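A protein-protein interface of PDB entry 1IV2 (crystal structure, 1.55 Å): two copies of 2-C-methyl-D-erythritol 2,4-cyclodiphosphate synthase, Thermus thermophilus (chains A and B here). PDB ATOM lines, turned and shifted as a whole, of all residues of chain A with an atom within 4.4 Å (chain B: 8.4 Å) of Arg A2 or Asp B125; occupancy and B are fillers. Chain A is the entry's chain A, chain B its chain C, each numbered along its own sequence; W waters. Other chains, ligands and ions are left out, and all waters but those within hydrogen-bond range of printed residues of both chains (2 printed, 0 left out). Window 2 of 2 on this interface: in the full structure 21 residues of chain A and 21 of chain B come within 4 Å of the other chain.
OD1 of Asp B125 is in salt-bridge range of NH2 of Arg A2, 2.5 Å away.
The backbone NH of Ile A3 sits close to the side-chain amide nitrogen of Gln B93.
OE1 of Gln B93 sits close to O of Ala A51 (2.9 Å).
O of Asp B125 lies close to O of Tyr A52, 3.5 Å away.
O of Ala A51 lies within hydrogen-bond range of NH1 of Arg A2.
O of Arg A2 sits at hydrogen-bond distance from N of Leu A150, at 2.9 Å.
N of Leu B92 lies within hydrogen-bond range of O of Leu B149 (2.7 Å).
NH1 of Arg B126 sits close to NE2 of Gln B93, 2.9 Å away.
N of Leu B149 lies within hydrogen-bond range of O of Gln B93 (2.9 Å).
O of Arg B126 sits at hydrogen-bond distance from N of Ala B94.
Among the printed residues, merely in contact across the chains: Arg A2 with Gln B93 (3.3 Å), Arg A2 with Arg B126 (3.4 Å), Ile A3 with Leu B149 (3.999 Å), Ala A51 with Asp B125 (3.8 Å), Gly A53 with Asp B125 (3.7 Å) and Gly A53 with Ile B127 (3.3 Å).
Of chain B, only Gln B93, Asp B125 and Arg B126 come within 4 Å of Arg A2.
Of chain A, only Arg A2, Ala A51, Tyr A52 and Gly A53 come within 4 Å of Asp B125.
Printed residues of chain B within 4 Å of Ala A51: Gln B93 and Asp B125.
Of the printed residues of chain B, Gly A53 touches Asp B125 and Ile B127.
Of the printed residues of chain A, Arg B126 touches Arg A2 (3.4 Å).
Of the printed residues of chain A, Ile B127 touches Gly A53 (3.3 Å).
Ala B94 touches none of the printed residues of chain A.
Ser B117 touches none of the printed residues of chain A.
The nearest residue of chain B that does not touch Arg A2 is Leu B149 (4.4 Å).
The nearest printed residue of chain A that does not touch Asp B125 is Ile A3 (7.2 Å).
Of the 15 printed residues of chain B, 5 touch a printed residue of chain A.
Hydrophobic or aromatic side chains of chain B that line the printed part of chain A: Leu B149.
Of the 8 printed residues of chain A, 5 touch a printed residue of chain B.
Printed residues of chain A that touch a printed residue of chain B: Arg A2, Ile A3, Ala A51, Tyr A52 and Gly A53.
Hydrophobic or aromatic side chains of chain A within 4 Å of the printed part of chain B: Ile A3.
Among the printed residues, 10 pairs touch across the chains.
Position printed for both chains: 149.
Water W2 bridges the backbone carbonyl oxygen of Gln B124 (2.6 Å) and the backbone carbonyl oxygen of Gly A53 (2.9 Å).
Water W1 lies within hydrogen-bond range of the guanidinium group of Arg B126 and the guanidinium group of Arg A2.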
ATOM      1  N   ARG A   2      -9.030 -11.039   1.697  1.00  0.00           N
ATOM      2  CA  ARG A   2      -8.594 -12.345   1.190  1.00  0.00           C
ATOM      3  C   ARG A   2      -9.551 -13.480   1.534  1.00  0.00           C
ATOM      4  O   ARG A   2     -10.160 -13.474   2.591  1.00  0.00           O
ATOM      5  CB  ARG A   2      -7.204 -12.688   1.739  1.00  0.00           C
ATOM      6  CG  ARG A   2      -6.088 -12.052   0.925  1.00  0.00           C
ATOM      7  CD  ARG A   2      -4.715 -12.593   1.346  1.00  0.00           C
ATOM      8  NE  ARG A   2      -3.712 -11.992   0.506  1.00  0.00           N
ATOM      9  CZ  ARG A   2      -2.928 -12.342  -0.466  1.00  0.00           C
ATOM     10  NH1 ARG A   2      -2.869 -13.558  -0.962  1.00  0.00           N
ATOM     11  NH2 ARG A   2      -2.139 -11.388  -0.955  1.00  0.00           N
ATOM     12  N   ILE A   3      -9.663 -14.445   0.629  1.00  0.00           N
ATOM     13  CA  ILE A   3     -10.554 -15.577   0.828  1.00  0.00           C
ATOM     14  C   ILE A   3      -9.781 -16.843   0.486  1.00  0.00           C
ATOM     15  O   ILE A   3      -8.881 -16.811  -0.353  1.00  0.00           O
ATOM     16  CB  ILE A   3     -11.811 -15.474  -0.048  1.00  0.00           C
ATOM     17  CG1 ILE A   3     -12.889 -16.519   0.260  1.00  0.00           C
ATOM     18  CG2 ILE A   3     -11.523 -15.557  -1.539  1.00  0.00           C
ATOM     19  CD1 ILE A   3     -14.136 -16.236  -0.572  1.00  0.00           C
ATOM     20  N   ALA A  51      -5.561 -19.145   0.640  1.00  0.00           N
ATOM     21  CA  ALA A  51      -5.774 -17.706   0.717  1.00  0.00           C
ATOM     22  C   ALA A  51      -4.489 -16.942   0.414  1.00  0.00           C
ATOM     23  O   ALA A  51      -4.579 -15.790   0.017  1.00  0.00           O
ATOM     24  CB  ALA A  51      -6.285 -17.341   2.101  1.00  0.00           C
ATOM     25  N   TYR A  52      -3.343 -17.587   0.622  1.00  0.00           N
ATOM     26  CA  TYR A  52      -2.091 -16.932   0.237  1.00  0.00           C
ATOM     27  C   TYR A  52      -1.373 -17.664  -0.876  1.00  0.00           C
ATOM     28  O   TYR A  52      -0.240 -17.330  -1.185  1.00  0.00           O
ATOM     29  CB  TYR A  52      -1.146 -16.789   1.447  1.00  0.00           C
ATOM     30  CG  TYR A  52      -1.526 -15.523   2.184  1.00  0.00           C
ATOM     31  CD1 TYR A  52      -2.583 -15.561   3.080  1.00  0.00           C
ATOM     32  CD2 TYR A  52      -0.860 -14.327   1.970  1.00  0.00           C
ATOM     33  CE1 TYR A  52      -2.958 -14.417   3.765  1.00  0.00           C
ATOM     34  CE2 TYR A  52      -1.234 -13.183   2.655  1.00  0.00           C
ATOM     35  CZ  TYR A  52      -2.280 -13.244   3.542  1.00  0.00           C
ATOM     36  OH  TYR A  52      -2.667 -12.121   4.234  1.00  0.00           O
ATOM     37  N   GLY A  53      -2.003 -18.649  -1.525  1.00  0.00           N
ATOM     38  CA  GLY A  53      -1.322 -19.289  -2.643  1.00  0.00           C
ATOM     39  C   GLY A  53      -0.161 -20.162  -2.174  1.00  0.00           C
ATOM     40  O   GLY A  53       0.746 -20.448  -2.973  1.00  0.00           O
ATOM     41  N   VAL A 148     -12.556 -19.458   4.219  1.00  0.00           N
ATOM     42  CA  VAL A 148     -12.020 -18.548   5.209  1.00  0.00           C
ATOM     43  C   VAL A 148     -11.961 -17.156   4.562  1.00  0.00           C
ATOM     44  O   VAL A 148     -11.835 -17.043   3.337  1.00  0.00           O
ATOM     45  CB  VAL A 148     -10.627 -18.928   5.766  1.00  0.00           C
ATOM     46  CG1 VAL A 148     -10.737 -20.191   6.614  1.00  0.00           C
ATOM     47  CG2 VAL A 148      -9.583 -19.095   4.667  1.00  0.00           C
ATOM     48  N   LEU A 149     -12.047 -16.203   5.478  1.00  0.00           N
ATOM     49  CA  LEU A 149     -12.005 -14.767   5.224  1.00  0.00           C
ATOM     50  C   LEU A 149     -10.907 -14.129   6.071  1.00  0.00           C
ATOM     51  O   LEU A 149     -10.868 -14.403   7.285  1.00  0.00           O
ATOM     52  CB  LEU A 149     -13.364 -14.156   5.555  1.00  0.00           C
ATOM     53  CG  LEU A 149     -13.552 -12.711   5.092  1.00  0.00           C
ATOM     54  CD1 LEU A 149     -13.352 -12.575   3.593  1.00  0.00           C
ATOM     55  CD2 LEU A 149     -14.937 -12.220   5.502  1.00  0.00           C
ATOM     56  N   LEU A 150     -10.056 -13.318   5.466  1.00  0.00           N
ATOM     57  CA  LEU A 150      -8.955 -12.711   6.228  1.00  0.00           C
ATOM     58  C   LEU A 150      -8.796 -11.233   5.858  1.00  0.00           C
ATOM     59  O   LEU A 150      -8.971 -10.910   4.691  1.00  0.00           O
ATOM     60  CB  LEU A 150      -7.638 -13.419   5.945  1.00  0.00           C
ATOM     61  CG  LEU A 150      -7.653 -14.935   6.146  1.00  0.00           C
ATOM     62  CD1 LEU A 150      -7.843 -15.593   4.786  1.00  0.00           C
ATOM     63  CD2 LEU A 150      -6.402 -15.408   6.853  1.00  0.00           C
ATOM     64  N   LEU B  92     -10.062  -9.990  -7.829  1.00  0.00           N
ATOM     65  CA  LEU B  92      -8.985  -9.885  -6.841  1.00  0.00           C
ATOM     66  C   LEU B  92      -8.352 -11.226  -6.477  1.00  0.00           C
ATOM     67  O   LEU B  92      -7.161 -11.237  -6.177  1.00  0.00           O
ATOM     68  CB  LEU B  92      -9.484  -9.182  -5.571  1.00  0.00           C
ATOM     69  CG  LEU B  92      -8.473  -9.224  -4.417  1.00  0.00           C
ATOM     70  CD1 LEU B  92      -7.364  -8.219  -4.677  1.00  0.00           C
ATOM     71  CD2 LEU B  92      -9.154  -8.968  -3.082  1.00  0.00           C
ATOM     72  N   GLN B  93      -9.121 -12.310  -6.524  1.00  0.00           N
ATOM     73  CA  GLN B  93      -8.608 -13.606  -6.089  1.00  0.00           C
ATOM     74  C   GLN B  93      -9.421 -14.778  -6.609  1.00  0.00           C
ATOM     75  O   GLN B  93     -10.635 -14.662  -6.814  1.00  0.00           O
ATOM     76  CB  GLN B  93      -8.633 -13.659  -4.546  1.00  0.00           C
ATOM     77  CG  GLN B  93      -7.796 -14.787  -3.964  1.00  0.00           C
ATOM     78  CD  GLN B  93      -7.514 -14.554  -2.488  1.00  0.00           C
ATOM     79  OE1 GLN B  93      -6.593 -15.163  -1.932  1.00  0.00           O
ATOM     80  NE2 GLN B  93      -8.289 -13.711  -1.832  1.00  0.00           N
ATOM     81  N   ALA B  94      -8.749 -15.910  -6.791  1.00  0.00           N
ATOM     82  CA  ALA B  94      -9.425 -17.165  -7.117  1.00  0.00           C
ATOM     83  C   ALA B  94      -8.868 -18.279  -6.233  1.00  0.00           C
ATOM     84  O   ALA B  94      -7.649 -18.432  -6.114  1.00  0.00           O
ATOM     85  CB  ALA B  94      -9.285 -17.514  -8.582  1.00  0.00           C
ATOM     86  N   SER B  95      -9.760 -19.045  -5.610  1.00  0.00           N
ATOM     87  CA  SER B  95      -9.327 -20.127  -4.724  1.00  0.00           C
ATOM     88  C   SER B  95     -10.154 -21.345  -5.094  1.00  0.00           C
ATOM     89  O   SER B  95     -11.377 -21.213  -5.011  1.00  0.00           O
ATOM     90  CB  SER B  95      -9.530 -19.782  -3.260  1.00  0.00           C
ATOM     91  OG  SER B  95      -9.065 -20.811  -2.409  1.00  0.00           O
ATOM     92  N   VAL B 113      -0.440 -23.309 -11.457  1.00  0.00           N
ATOM     93  CA  VAL B 113      -0.694 -22.015 -10.833  1.00  0.00           C
ATOM     94  C   VAL B 113      -0.260 -20.907 -11.773  1.00  0.00           C
ATOM     95  O   VAL B 113      -0.999 -19.931 -11.914  1.00  0.00           O
ATOM     96  CB  VAL B 113       0.031 -21.927  -9.481  1.00  0.00           C
ATOM     97  CG1 VAL B 113      -0.039 -20.500  -8.945  1.00  0.00           C
ATOM     98  CG2 VAL B 113      -0.599 -22.907  -8.513  1.00  0.00           C
ATOM     99  N   SER B 117      -2.585 -17.864 -13.127  1.00  0.00           N
ATOM    100  CA  SER B 117      -2.106 -16.522 -12.878  1.00  0.00           C
ATOM    101  C   SER B 117      -2.135 -15.666 -14.134  1.00  0.00           C
ATOM    102  O   SER B 117      -2.511 -14.499 -14.193  1.00  0.00           O
ATOM    103  CB  SER B 117      -0.652 -16.618 -12.364  1.00  0.00           C
ATOM    104  OG  SER B 117      -0.148 -15.296 -12.251  1.00  0.00           O
ATOM    105  N   LEU B 122      -3.783 -12.507 -12.411  1.00  0.00           N
ATOM    106  CA  LEU B 122      -3.651 -12.318 -10.978  1.00  0.00           C
ATOM    107  C   LEU B 122      -2.244 -12.669 -10.515  1.00  0.00           C
ATOM    108  O   LEU B 122      -1.637 -13.590 -11.066  1.00  0.00           O
ATOM    109  CB  LEU B 122      -4.626 -13.207 -10.190  1.00  0.00           C
ATOM    110  CG  LEU B 122      -6.115 -12.854 -10.346  1.00  0.00           C
ATOM    111  CD1 LEU B 122      -6.959 -13.866  -9.594  1.00  0.00           C
ATOM    112  CD2 LEU B 122      -6.420 -11.446  -9.855  1.00  0.00           C
ATOM    113  N   PRO B 123      -1.772 -11.960  -9.501  1.00  0.00           N
ATOM    114  CA  PRO B 123      -0.489 -12.332  -8.877  1.00  0.00           C
ATOM    115  C   PRO B 123      -0.571 -13.741  -8.292  1.00  0.00           C
ATOM    116  O   PRO B 123      -1.654 -14.188  -7.888  1.00  0.00           O
ATOM    117  CB  PRO B 123      -0.298 -11.302  -7.766  1.00  0.00           C
ATOM    118  CG  PRO B 123      -1.622 -10.677  -7.558  1.00  0.00           C
ATOM    119  CD  PRO B 123      -2.389 -10.795  -8.859  1.00  0.00           C
ATOM    120  N   GLN B 124       0.570 -14.433  -8.217  1.00  0.00           N
ATOM    121  CA  GLN B 124       0.488 -15.848  -7.838  1.00  0.00           C
ATOM    122  C   GLN B 124      -0.029 -16.090  -6.433  1.00  0.00           C
ATOM    123  O   GLN B 124      -0.584 -17.167  -6.145  1.00  0.00           O
ATOM    124  CB  GLN B 124       1.861 -16.513  -8.014  1.00  0.00           C
ATOM    125  CG  GLN B 124       2.338 -16.371  -9.461  1.00  0.00           C
ATOM    126  CD  GLN B 124       2.934 -17.636 -10.031  1.00  0.00           C
ATOM    127  OE1 GLN B 124       3.153 -18.646  -9.361  1.00  0.00           O
ATOM    128  NE2 GLN B 124       3.233 -17.604 -11.325  1.00  0.00           N
ATOM    129  N   ASP B 125       0.140 -15.118  -5.537  1.00  0.00           N
ATOM    130  CA  ASP B 125      -0.322 -15.315  -4.179  1.00  0.00           C
ATOM    131  C   ASP B 125      -1.841 -15.115  -4.100  1.00  0.00           C
ATOM    132  O   ASP B 125      -2.396 -15.312  -3.017  1.00  0.00           O
ATOM    133  CB  ASP B 125       0.375 -14.324  -3.234  1.00  0.00           C
ATOM    134  CG  ASP B 125      -0.073 -12.919  -3.648  1.00  0.00           C
ATOM    135  OD1 ASP B 125      -0.811 -12.291  -2.869  1.00  0.00           O
ATOM    136  OD2 ASP B 125       0.310 -12.509  -4.765  1.00  0.00           O
ATOM    137  N   ARG B 126      -2.444 -14.731  -5.230  1.00  0.00           N
ATOM    138  CA  ARG B 126      -3.891 -14.562  -5.324  1.00  0.00           C
ATOM    139  C   ARG B 126      -4.558 -15.687  -6.120  1.00  0.00           C
ATOM    140  O   ARG B 126      -5.754 -15.619  -6.423  1.00  0.00           O
ATOM    141  CB  ARG B 126      -4.223 -13.197  -5.949  1.00  0.00           C
ATOM    142  CG  ARG B 126      -3.908 -12.037  -5.005  1.00  0.00           C
ATOM    143  CD  ARG B 126      -4.889 -12.033  -3.843  1.00  0.00           C
ATOM    144  NE  ARG B 126      -4.941 -10.780  -3.110  1.00  0.00           N
ATOM    145  CZ  ARG B 126      -5.952 -10.389  -2.346  1.00  0.00           C
ATOM    146  NH1 ARG B 126      -7.046 -11.115  -2.175  1.00  0.00           N
ATOM    147  NH2 ARG B 126      -5.871  -9.214  -1.729  1.00  0.00           N
ATOM    148  N   ILE B 127      -3.764 -16.694  -6.441  1.00  0.00           N
ATOM    149  CA  ILE B 127      -4.194 -17.955  -7.042  1.00  0.00           C
ATOM    150  C   ILE B 127      -4.044 -19.017  -5.947  1.00  0.00           C
ATOM    151  O   ILE B 127      -2.937 -19.395  -5.542  1.00  0.00           O
ATOM    152  CB  ILE B 127      -3.418 -18.383  -8.294  1.00  0.00           C
ATOM    153  CG1 ILE B 127      -3.475 -17.399  -9.475  1.00  0.00           C
ATOM    154  CG2 ILE B 127      -3.835 -19.779  -8.752  1.00  0.00           C
ATOM    155  CD1 ILE B 127      -4.885 -17.178 -10.007  1.00  0.00           C
ATOM    156  N   GLY B 128      -5.183 -19.465  -5.439  1.00  0.00           N
ATOM    157  CA  GLY B 128      -5.180 -20.454  -4.362  1.00  0.00           C
ATOM    158  C   GLY B 128      -5.604 -21.795  -4.930  1.00  0.00           C
ATOM    159  O   GLY B 128      -6.798 -21.983  -5.149  1.00  0.00           O
ATOM    160  N   LEU B 129      -4.659 -22.685  -5.191  1.00  0.00           N
ATOM    161  CA  LEU B 129      -4.980 -23.966  -5.799  1.00  0.00           C
ATOM    162  C   LEU B 129      -4.511 -25.070  -4.853  1.00  0.00           C
ATOM    163  O   LEU B 129      -3.334 -25.094  -4.427  1.00  0.00           O
ATOM    164  CB  LEU B 129      -4.332 -24.086  -7.185  1.00  0.00           C
ATOM    165  CG  LEU B 129      -4.535 -25.391  -7.956  1.00  0.00           C
ATOM    166  CD1 LEU B 129      -5.979 -25.619  -8.413  1.00  0.00           C
ATOM    167  CD2 LEU B 129      -3.591 -25.437  -9.166  1.00  0.00           C
ATOM    168  N   LEU B 149     -13.187 -13.715  -5.789  1.00  0.00           N
ATOM    169  CA  LEU B 149     -13.425 -12.470  -5.062  1.00  0.00           C
ATOM    170  C   LEU B 149     -13.091 -11.299  -5.976  1.00  0.00           C
ATOM    171  O   LEU B 149     -12.025 -11.348  -6.605  1.00  0.00           O
ATOM    172  CB  LEU B 149     -12.581 -12.434  -3.802  1.00  0.00           C
ATOM    173  CG  LEU B 149     -12.665 -11.171  -2.948  1.00  0.00           C
ATOM    174  CD1 LEU B 149     -14.019 -11.098  -2.267  1.00  0.00           C
ATOM    175  CD2 LEU B 149     -11.541 -11.152  -1.925  1.00  0.00           C
HETATM  176  O   HOH W   1      -2.691  -9.367  -3.541  1.00  0.00           O
HETATM  177  O   HOH W   2       1.154 -18.941  -5.471  1.00  0.00           O
